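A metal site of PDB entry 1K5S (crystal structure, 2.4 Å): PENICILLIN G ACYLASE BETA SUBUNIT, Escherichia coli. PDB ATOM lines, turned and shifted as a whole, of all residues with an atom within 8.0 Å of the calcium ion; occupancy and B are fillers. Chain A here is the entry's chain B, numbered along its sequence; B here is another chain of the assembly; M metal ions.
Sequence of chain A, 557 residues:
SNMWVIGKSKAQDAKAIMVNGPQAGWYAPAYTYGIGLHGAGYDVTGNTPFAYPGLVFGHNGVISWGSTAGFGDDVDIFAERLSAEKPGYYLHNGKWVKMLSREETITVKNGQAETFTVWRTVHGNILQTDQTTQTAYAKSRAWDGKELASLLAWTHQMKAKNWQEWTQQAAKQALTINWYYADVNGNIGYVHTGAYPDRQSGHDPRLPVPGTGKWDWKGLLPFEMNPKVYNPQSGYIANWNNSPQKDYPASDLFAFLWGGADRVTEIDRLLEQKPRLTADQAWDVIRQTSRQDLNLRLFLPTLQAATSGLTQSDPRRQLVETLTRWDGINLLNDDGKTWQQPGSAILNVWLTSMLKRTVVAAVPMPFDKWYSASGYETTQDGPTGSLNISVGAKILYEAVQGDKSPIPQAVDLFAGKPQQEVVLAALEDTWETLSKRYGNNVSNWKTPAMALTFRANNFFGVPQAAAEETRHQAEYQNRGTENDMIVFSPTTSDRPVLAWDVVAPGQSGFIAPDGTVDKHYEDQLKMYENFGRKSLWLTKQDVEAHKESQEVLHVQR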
ATOM      1  N   GLY A  72      10.560  25.913 -33.667  1.00  0.00           N
ATOM      2  CA  GLY A  72      11.323  26.122 -32.447  1.00  0.00           C
ATOM      3  C   GLY A  72      10.379  25.763 -31.311  1.00  0.00           C
ATOM      4  O   GLY A  72       9.183  25.535 -31.537  1.00  0.00           O
ATOM      5  N   ASP A  73      10.901  25.684 -30.098  1.00  0.00           N
ATOM      6  CA  ASP A  73      10.076  25.390 -28.941  1.00  0.00           C
ATOM      7  C   ASP A  73       9.521  26.697 -28.370  1.00  0.00           C
ATOM      8  O   ASP A  73      10.184  27.377 -27.573  1.00  0.00           O
ATOM      9  CB  ASP A  73      10.869  24.641 -27.880  1.00  0.00           C
ATOM     10  CG  ASP A  73       9.993  24.080 -26.760  1.00  0.00           C
ATOM     11  OD1 ASP A  73       8.809  24.496 -26.663  1.00  0.00           O
ATOM     12  OD2 ASP A  73      10.394  23.206 -25.944  1.00  0.00           O
ATOM     13  N   ASP A  74       8.297  27.056 -28.768  1.00  0.00           N
ATOM     14  CA  ASP A  74       7.687  28.296 -28.274  1.00  0.00           C
ATOM     15  C   ASP A  74       6.408  28.007 -27.483  1.00  0.00           C
ATOM     16  O   ASP A  74       5.639  28.920 -27.196  1.00  0.00           O
ATOM     17  CB  ASP A  74       7.396  29.237 -29.439  1.00  0.00           C
ATOM     18  CG  ASP A  74       6.453  28.616 -30.479  1.00  0.00           C
ATOM     19  OD1 ASP A  74       6.170  27.415 -30.388  1.00  0.00           O
ATOM     20  OD2 ASP A  74       5.929  29.271 -31.399  1.00  0.00           O
ATOM     21  N   VAL A  75       6.216  26.729 -27.128  1.00  0.00           N
ATOM     22  CA  VAL A  75       5.035  26.270 -26.380  1.00  0.00           C
ATOM     23  C   VAL A  75       5.389  25.365 -25.192  1.00  0.00           C
ATOM     24  O   VAL A  75       6.073  24.354 -25.345  1.00  0.00           O
ATOM     25  CB  VAL A  75       4.089  25.475 -27.283  1.00  0.00           C
ATOM     26  CG1 VAL A  75       2.850  25.051 -26.519  1.00  0.00           C
ATOM     27  CG2 VAL A  75       3.710  26.279 -28.525  1.00  0.00           C
ATOM     28  N   ASP A  76       4.929  25.739 -24.012  1.00  0.00           N
ATOM     29  CA  ASP A  76       5.150  24.943 -22.821  1.00  0.00           C
ATOM     30  C   ASP A  76       3.786  24.623 -22.163  1.00  0.00           C
ATOM     31  O   ASP A  76       2.806  25.375 -22.317  1.00  0.00           O
ATOM     32  CB  ASP A  76       6.045  25.695 -21.812  1.00  0.00           C
ATOM     33  CG  ASP A  76       7.511  25.805 -22.279  1.00  0.00           C
ATOM     34  OD1 ASP A  76       7.976  24.996 -23.131  1.00  0.00           O
ATOM     35  OD2 ASP A  76       8.274  26.699 -21.817  1.00  0.00           O
ATOM     36  N   ILE A  77       3.733  23.519 -21.426  1.00  0.00           N
ATOM     37  CA  ILE A  77       2.500  23.111 -20.784  1.00  0.00           C
ATOM     38  C   ILE A  77       2.631  23.258 -19.265  1.00  0.00           C
ATOM     39  O   ILE A  77       3.584  22.742 -18.663  1.00  0.00           O
ATOM     40  CB  ILE A  77       2.178  21.646 -21.150  1.00  0.00           C
ATOM     41  CG1 ILE A  77       1.717  21.539 -22.614  1.00  0.00           C
ATOM     42  CG2 ILE A  77       1.129  21.076 -20.211  1.00  0.00           C
ATOM     43  CD1 ILE A  77       1.309  20.136 -23.033  1.00  0.00           C
ATOM     44  N   SER A 140       0.615  26.846 -22.940  1.00  0.00           N
ATOM     45  CA  SER A 140       1.154  28.201 -22.967  1.00  0.00           C
ATOM     46  C   SER A 140       1.997  28.536 -24.202  1.00  0.00           C
ATOM     47  O   SER A 140       3.038  27.928 -24.428  1.00  0.00           O
ATOM     48  CB  SER A 140       1.963  28.432 -21.698  1.00  0.00           C
ATOM     49  OG  SER A 140       2.215  29.804 -21.498  1.00  0.00           O
ATOM     50  N   PRO A 197      10.115  32.089 -25.061  1.00  0.00           N
ATOM     51  CA  PRO A 197      10.090  32.362 -23.622  1.00  0.00           C
ATOM     52  C   PRO A 197      11.461  32.369 -22.939  1.00  0.00           C
ATOM     53  O   PRO A 197      12.371  31.609 -23.308  1.00  0.00           O
ATOM     54  CB  PRO A 197       9.226  31.217 -23.058  1.00  0.00           C
ATOM     55  CG  PRO A 197       9.444  30.114 -24.030  1.00  0.00           C
ATOM     56  CD  PRO A 197       9.522  30.774 -25.384  1.00  0.00           C
ATOM     57  N   ARG A 199      13.058  31.310 -19.891  1.00  0.00           N
ATOM     58  CA  ARG A 199      12.649  30.313 -18.901  1.00  0.00           C
ATOM     59  C   ARG A 199      13.444  30.337 -17.598  1.00  0.00           C
ATOM     60  O   ARG A 199      14.616  30.712 -17.577  1.00  0.00           O
ATOM     61  CB  ARG A 199      12.714  28.915 -19.512  1.00  0.00           C
ATOM     62  CG  ARG A 199      11.789  28.696 -20.716  1.00  0.00           C
ATOM     63  CD  ARG A 199      11.880  27.274 -21.289  1.00  0.00           C
ATOM     64  NE  ARG A 199      10.890  26.963 -22.322  1.00  0.00           N
ATOM     65  CZ  ARG A 199      11.094  27.045 -23.639  1.00  0.00           C
ATOM     66  NH1 ARG A 199      12.259  27.435 -24.145  1.00  0.00           N
ATOM     67  NH2 ARG A 199      10.117  26.713 -24.461  1.00  0.00           N
ATOM     68  N   HIS A 203      14.516  24.832 -15.976  1.00  0.00           N
ATOM     69  CA  HIS A 203      13.311  24.450 -16.709  1.00  0.00           C
ATOM     70  C   HIS A 203      13.661  23.628 -17.930  1.00  0.00           C
ATOM     71  O   HIS A 203      14.327  24.109 -18.850  1.00  0.00           O
ATOM     72  CB  HIS A 203      12.529  25.725 -17.104  1.00  0.00           C
ATOM     73  CG  HIS A 203      11.269  25.487 -17.886  1.00  0.00           C
ATOM     74  ND1 HIS A 203      10.284  26.443 -18.013  1.00  0.00           N
ATOM     75  CD2 HIS A 203      10.833  24.404 -18.583  1.00  0.00           C
ATOM     76  CE1 HIS A 203       9.307  25.973 -18.770  1.00  0.00           C
ATOM     77  NE2 HIS A 203       9.612  24.741 -19.130  1.00  0.00           N
ATOM     78  N   ASP A 204      13.220  22.376 -17.958  1.00  0.00           N
ATOM     79  CA  ASP A 204      13.453  21.509 -19.104  1.00  0.00           C
ATOM     80  C   ASP A 204      12.297  21.750 -20.061  1.00  0.00           C
ATOM     81  O   ASP A 204      11.197  21.317 -19.779  1.00  0.00           O
ATOM     82  CB  ASP A 204      13.460  20.043 -18.665  1.00  0.00           C
ATOM     83  CG  ASP A 204      13.992  19.122 -19.738  1.00  0.00           C
ATOM     84  OD1 ASP A 204      13.602  19.281 -20.901  1.00  0.00           O
ATOM     85  OD2 ASP A 204      14.816  18.208 -19.486  1.00  0.00           O
ATOM     86  N   PRO A 205      12.559  22.390 -21.191  1.00  0.00           N
ATOM     87  CA  PRO A 205      11.498  22.805 -22.130  1.00  0.00           C
ATOM     88  C   PRO A 205      10.865  21.634 -22.868  1.00  0.00           C
ATOM     89  O   PRO A 205      10.072  21.845 -23.763  1.00  0.00           O
ATOM     90  CB  PRO A 205      12.257  23.704 -23.088  1.00  0.00           C
ATOM     91  CG  PRO A 205      13.587  23.012 -23.165  1.00  0.00           C
ATOM     92  CD  PRO A 205      13.904  22.709 -21.711  1.00  0.00           C
ATOM     93  N   ARG A 206      11.222  20.415 -22.499  1.00  0.00           N
ATOM     94  CA  ARG A 206      10.684  19.225 -23.155  1.00  0.00           C
ATOM     95  C   ARG A 206       9.603  18.587 -22.301  1.00  0.00           C
ATOM     96  O   ARG A 206       8.912  17.674 -22.750  1.00  0.00           O
ATOM     97  CB  ARG A 206      11.792  18.213 -23.390  1.00  0.00           C
ATOM     98  CG  ARG A 206      12.901  18.721 -24.292  1.00  0.00           C
ATOM     99  CD  ARG A 206      14.057  17.768 -24.367  1.00  0.00           C
ATOM    100  NE  ARG A 206      14.599  17.536 -23.038  1.00  0.00           N
ATOM    101  CZ  ARG A 206      15.546  16.660 -22.776  1.00  0.00           C
ATOM    102  NH1 ARG A 206      16.057  15.927 -23.766  1.00  0.00           N
ATOM    103  NH2 ARG A 206      15.977  16.510 -21.527  1.00  0.00           N
ATOM    104  N   LEU A 207       9.466  19.076 -21.074  1.00  0.00           N
ATOM    105  CA  LEU A 207       8.538  18.469 -20.132  1.00  0.00           C
ATOM    106  C   LEU A 207       7.699  19.522 -19.408  1.00  0.00           C
ATOM    107  O   LEU A 207       8.105  20.674 -19.317  1.00  0.00           O
ATOM    108  CB  LEU A 207       9.327  17.603 -19.150  1.00  0.00           C
ATOM    109  CG  LEU A 207      10.142  16.557 -19.906  1.00  0.00           C
ATOM    110  CD1 LEU A 207      11.337  16.015 -19.151  1.00  0.00           C
ATOM    111  CD2 LEU A 207       9.228  15.416 -20.347  1.00  0.00           C
ATOM    112  N   PRO A 208       6.533  19.135 -18.933  1.00  0.00           N
ATOM    113  CA  PRO A 208       5.635  20.068 -18.233  1.00  0.00           C
ATOM    114  C   PRO A 208       6.253  20.727 -17.006  1.00  0.00           C
ATOM    115  O   PRO A 208       7.183  20.195 -16.392  1.00  0.00           O
ATOM    116  CB  PRO A 208       4.485  19.168 -17.796  1.00  0.00           C
ATOM    117  CG  PRO A 208       4.490  18.051 -18.749  1.00  0.00           C
ATOM    118  CD  PRO A 208       5.954  17.782 -19.041  1.00  0.00           C
ATOM    119  N   TRP A 217       7.202  31.776 -16.805  1.00  0.00           N
ATOM    120  CA  TRP A 217       8.269  32.348 -17.611  1.00  0.00           C
ATOM    121  C   TRP A 217       8.689  33.703 -17.036  1.00  0.00           C
ATOM    122  O   TRP A 217       7.918  34.351 -16.323  1.00  0.00           O
ATOM    123  CB  TRP A 217       7.812  32.496 -19.059  1.00  0.00           C
ATOM    124  CG  TRP A 217       7.508  31.200 -19.790  1.00  0.00           C
ATOM    125  CD1 TRP A 217       7.986  29.963 -19.509  1.00  0.00           C
ATOM    126  CD2 TRP A 217       6.668  31.061 -20.929  1.00  0.00           C
ATOM    127  NE1 TRP A 217       7.503  29.047 -20.418  1.00  0.00           N
ATOM    128  CE2 TRP A 217       6.680  29.699 -21.294  1.00  0.00           C
ATOM    129  CE3 TRP A 217       5.917  31.947 -21.713  1.00  0.00           C
ATOM    130  CZ2 TRP A 217       5.976  29.211 -22.389  1.00  0.00           C
ATOM    131  CZ3 TRP A 217       5.202  31.458 -22.789  1.00  0.00           C
ATOM    132  CH2 TRP A 217       5.243  30.097 -23.117  1.00  0.00           C
ATOM    133  N   ALA A 250      15.166  22.555 -30.818  1.00  0.00           N
ATOM    134  CA  ALA A 250      13.997  22.256 -31.610  1.00  0.00           C
ATOM    135  C   ALA A 250      12.729  22.161 -30.795  1.00  0.00           C
ATOM    136  O   ALA A 250      12.748  22.123 -29.571  1.00  0.00           O
ATOM    137  CB  ALA A 250      14.201  20.947 -32.362  1.00  0.00           C
ATOM    138  N   SER A 251      11.619  22.119 -31.521  1.00  0.00           N
ATOM    139  CA  SER A 251      10.296  21.863 -30.972  1.00  0.00           C
ATOM    140  C   SER A 251      10.349  20.678 -30.014  1.00  0.00           C
ATOM    141  O   SER A 251      11.192  19.778 -30.166  1.00  0.00           O
ATOM    142  CB  SER A 251       9.363  21.535 -32.134  1.00  0.00           C
ATOM    143  OG  SER A 251       8.106  21.122 -31.660  1.00  0.00           O
ATOM    144  N   ASP A 252       9.448  20.647 -29.035  1.00  0.00           N
ATOM    145  CA  ASP A 252       9.435  19.527 -28.082  1.00  0.00           C
ATOM    146  C   ASP A 252       8.752  18.258 -28.605  1.00  0.00           C
ATOM    147  O   ASP A 252       8.709  17.263 -27.888  1.00  0.00           O
ATOM    148  CB  ASP A 252       8.891  19.958 -26.706  1.00  0.00           C
ATOM    149  CG  ASP A 252       7.426  20.322 -26.735  1.00  0.00           C
ATOM    150  OD1 ASP A 252       6.617  19.564 -27.323  1.00  0.00           O
ATOM    151  OD2 ASP A 252       6.978  21.342 -26.197  1.00  0.00           O
ATOM    152  N   LEU A 253       8.256  18.270 -29.831  1.00  0.00           N
ATOM    153  CA  LEU A 253       7.591  17.092 -30.402  1.00  0.00           C
ATOM    154  C   LEU A 253       8.484  15.854 -30.378  1.00  0.00           C
ATOM    155  O   LEU A 253       9.604  15.887 -30.881  1.00  0.00           O
ATOM    156  CB  LEU A 253       7.123  17.346 -31.832  1.00  0.00           C
ATOM    157  CG  LEU A 253       6.060  18.427 -31.986  1.00  0.00           C
ATOM    158  CD1 LEU A 253       5.707  18.665 -33.471  1.00  0.00           C
ATOM    159  CD2 LEU A 253       4.844  18.029 -31.175  1.00  0.00           C
ATOM    160  N   SER B 150       2.691  23.599 -31.642  1.00  0.00           N
ATOM    161  CA  SER B 150       3.096  22.201 -31.467  1.00  0.00           C
ATOM    162  C   SER B 150       3.790  21.886 -30.139  1.00  0.00           C
ATOM    163  O   SER B 150       4.799  22.501 -29.797  1.00  0.00           O
ATOM    164  CB  SER B 150       4.018  21.802 -32.603  1.00  0.00           C
ATOM    165  OG  SER B 150       3.716  22.496 -33.791  1.00  0.00           O
ATOM    166  N   THR B 151       3.266  20.896 -29.422  1.00  0.00           N
ATOM    167  CA  THR B 151       3.886  20.417 -28.191  1.00  0.00           C
ATOM    168  C   THR B 151       3.387  19.023 -27.827  1.00  0.00           C
ATOM    169  O   THR B 151       2.210  18.706 -28.010  1.00  0.00           O
ATOM    170  CB  THR B 151       3.604  21.407 -27.035  1.00  0.00           C
ATOM    171  OG1 THR B 151       4.403  21.069 -25.896  1.00  0.00           O
ATOM    172  CG2 THR B 151       2.160  21.252 -26.539  1.00  0.00           C
ATOM    173  N   SER B 152       4.290  18.182 -27.329  1.00  0.00           N
ATOM    174  CA  SER B 152       3.920  16.836 -26.874  1.00  0.00           C
ATOM    175  C   SER B 152       4.535  16.593 -25.495  1.00  0.00           C
ATOM    176  O   SER B 152       4.897  15.460 -25.146  1.00  0.00           O
ATOM    177  CB  SER B 152       4.423  15.782 -27.851  1.00  0.00           C
ATOM    178  OG  SER B 152       5.838  15.680 -27.791  1.00  0.00           O
ATOM    179  N   GLU B 153       4.665  17.675 -24.722  1.00  0.00           N
ATOM    180  CA  GLU B 153       5.263  17.616 -23.392  1.00  0.00           C
ATOM    181  C   GLU B 153       4.679  16.564 -22.438  1.00  0.00           C
ATOM    182  O   GLU B 153       5.411  15.940 -21.671  1.00  0.00           O
ATOM    183  CB  GLU B 153       5.226  18.994 -22.731  1.00  0.00           C
ATOM    184  CG  GLU B 153       6.433  19.847 -23.048  1.00  0.00           C
ATOM    185  CD  GLU B 153       6.377  21.223 -22.434  1.00  0.00           C
ATOM    186  OE1 GLU B 153       5.737  21.388 -21.373  1.00  0.00           O
ATOM    187  OE2 GLU B 153       6.980  22.146 -23.024  1.00  0.00           O
ATOM    188  N   ASN B 156       5.843  13.207 -23.727  1.00  0.00           N
ATOM    189  CA  ASN B 156       7.250  13.155 -23.409  1.00  0.00           C
ATOM    190  C   ASN B 156       7.487  12.749 -21.953  1.00  0.00           C
ATOM    191  O   ASN B 156       8.375  11.941 -21.661  1.00  0.00           O
ATOM    192  CB  ASN B 156       7.916  14.507 -23.669  1.00  0.00           C
ATOM    193  CG  ASN B 156       7.840  14.957 -25.128  1.00  0.00           C
ATOM    194  OD1 ASN B 156       7.419  14.206 -26.028  1.00  0.00           O
ATOM    195  ND2 ASN B 156       8.246  16.205 -25.357  1.00  0.00           N
HETATM  196 CA    CA M   1       8.090  23.126 -24.606  1.00  0.00          CA
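N of Ser 140 lies within hydrogen-bond range of O of Asp 76.
ND2 of Asn 156 of chain B lies within hydrogen-bond range of O of Asp 252 (2.8 Å).
The backbone carbonyl oxygen of Asp 73 lies within hydrogen-bond range of the guanidinium group of Arg 199.
OD1 of Asp 252 lies close to OG1 of Thr 151 of chain B (3.0 Å).
The side-chain carboxylate (OE1) of Glu 153 of chain B is in hydrogen-bond range of the backbone NH (N) of Ile 77, at 2.9 Å.
The guanidinium group of Arg 199 lies within salt-bridge range of the side-chain carboxylate of Asp 76 (2.7 Å).
OD1 of Asp 252 sits at hydrogen-bond distance from N of Ser 152 of chain B (2.7 Å).
NE1 of Trp 217 lies within hydrogen-bond range of OD2 of Asp 76, at 2.8 Å.
The calcium ion is bound by OE2 of Glu 153 of chain B, at 2.2 Å.
The calcium ion is bound by OD1 of Asp 76 (2.4 Å).
The calcium ion is bound by O of Val 75.
O of Pro 205 is bound to the calcium ion, 2.5 Å away.
The calcium ion is bound by OD1 of Asp 73.
OD2 of Asp 252 binds the calcium ion, at 2.6 Å.
The calcium ion is bound by the side-chain carboxylate (OD2) of Asp 73, at 2.7 Å.
Of the 25 residues printed, 6 come within 4 Å of the calcium ion.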
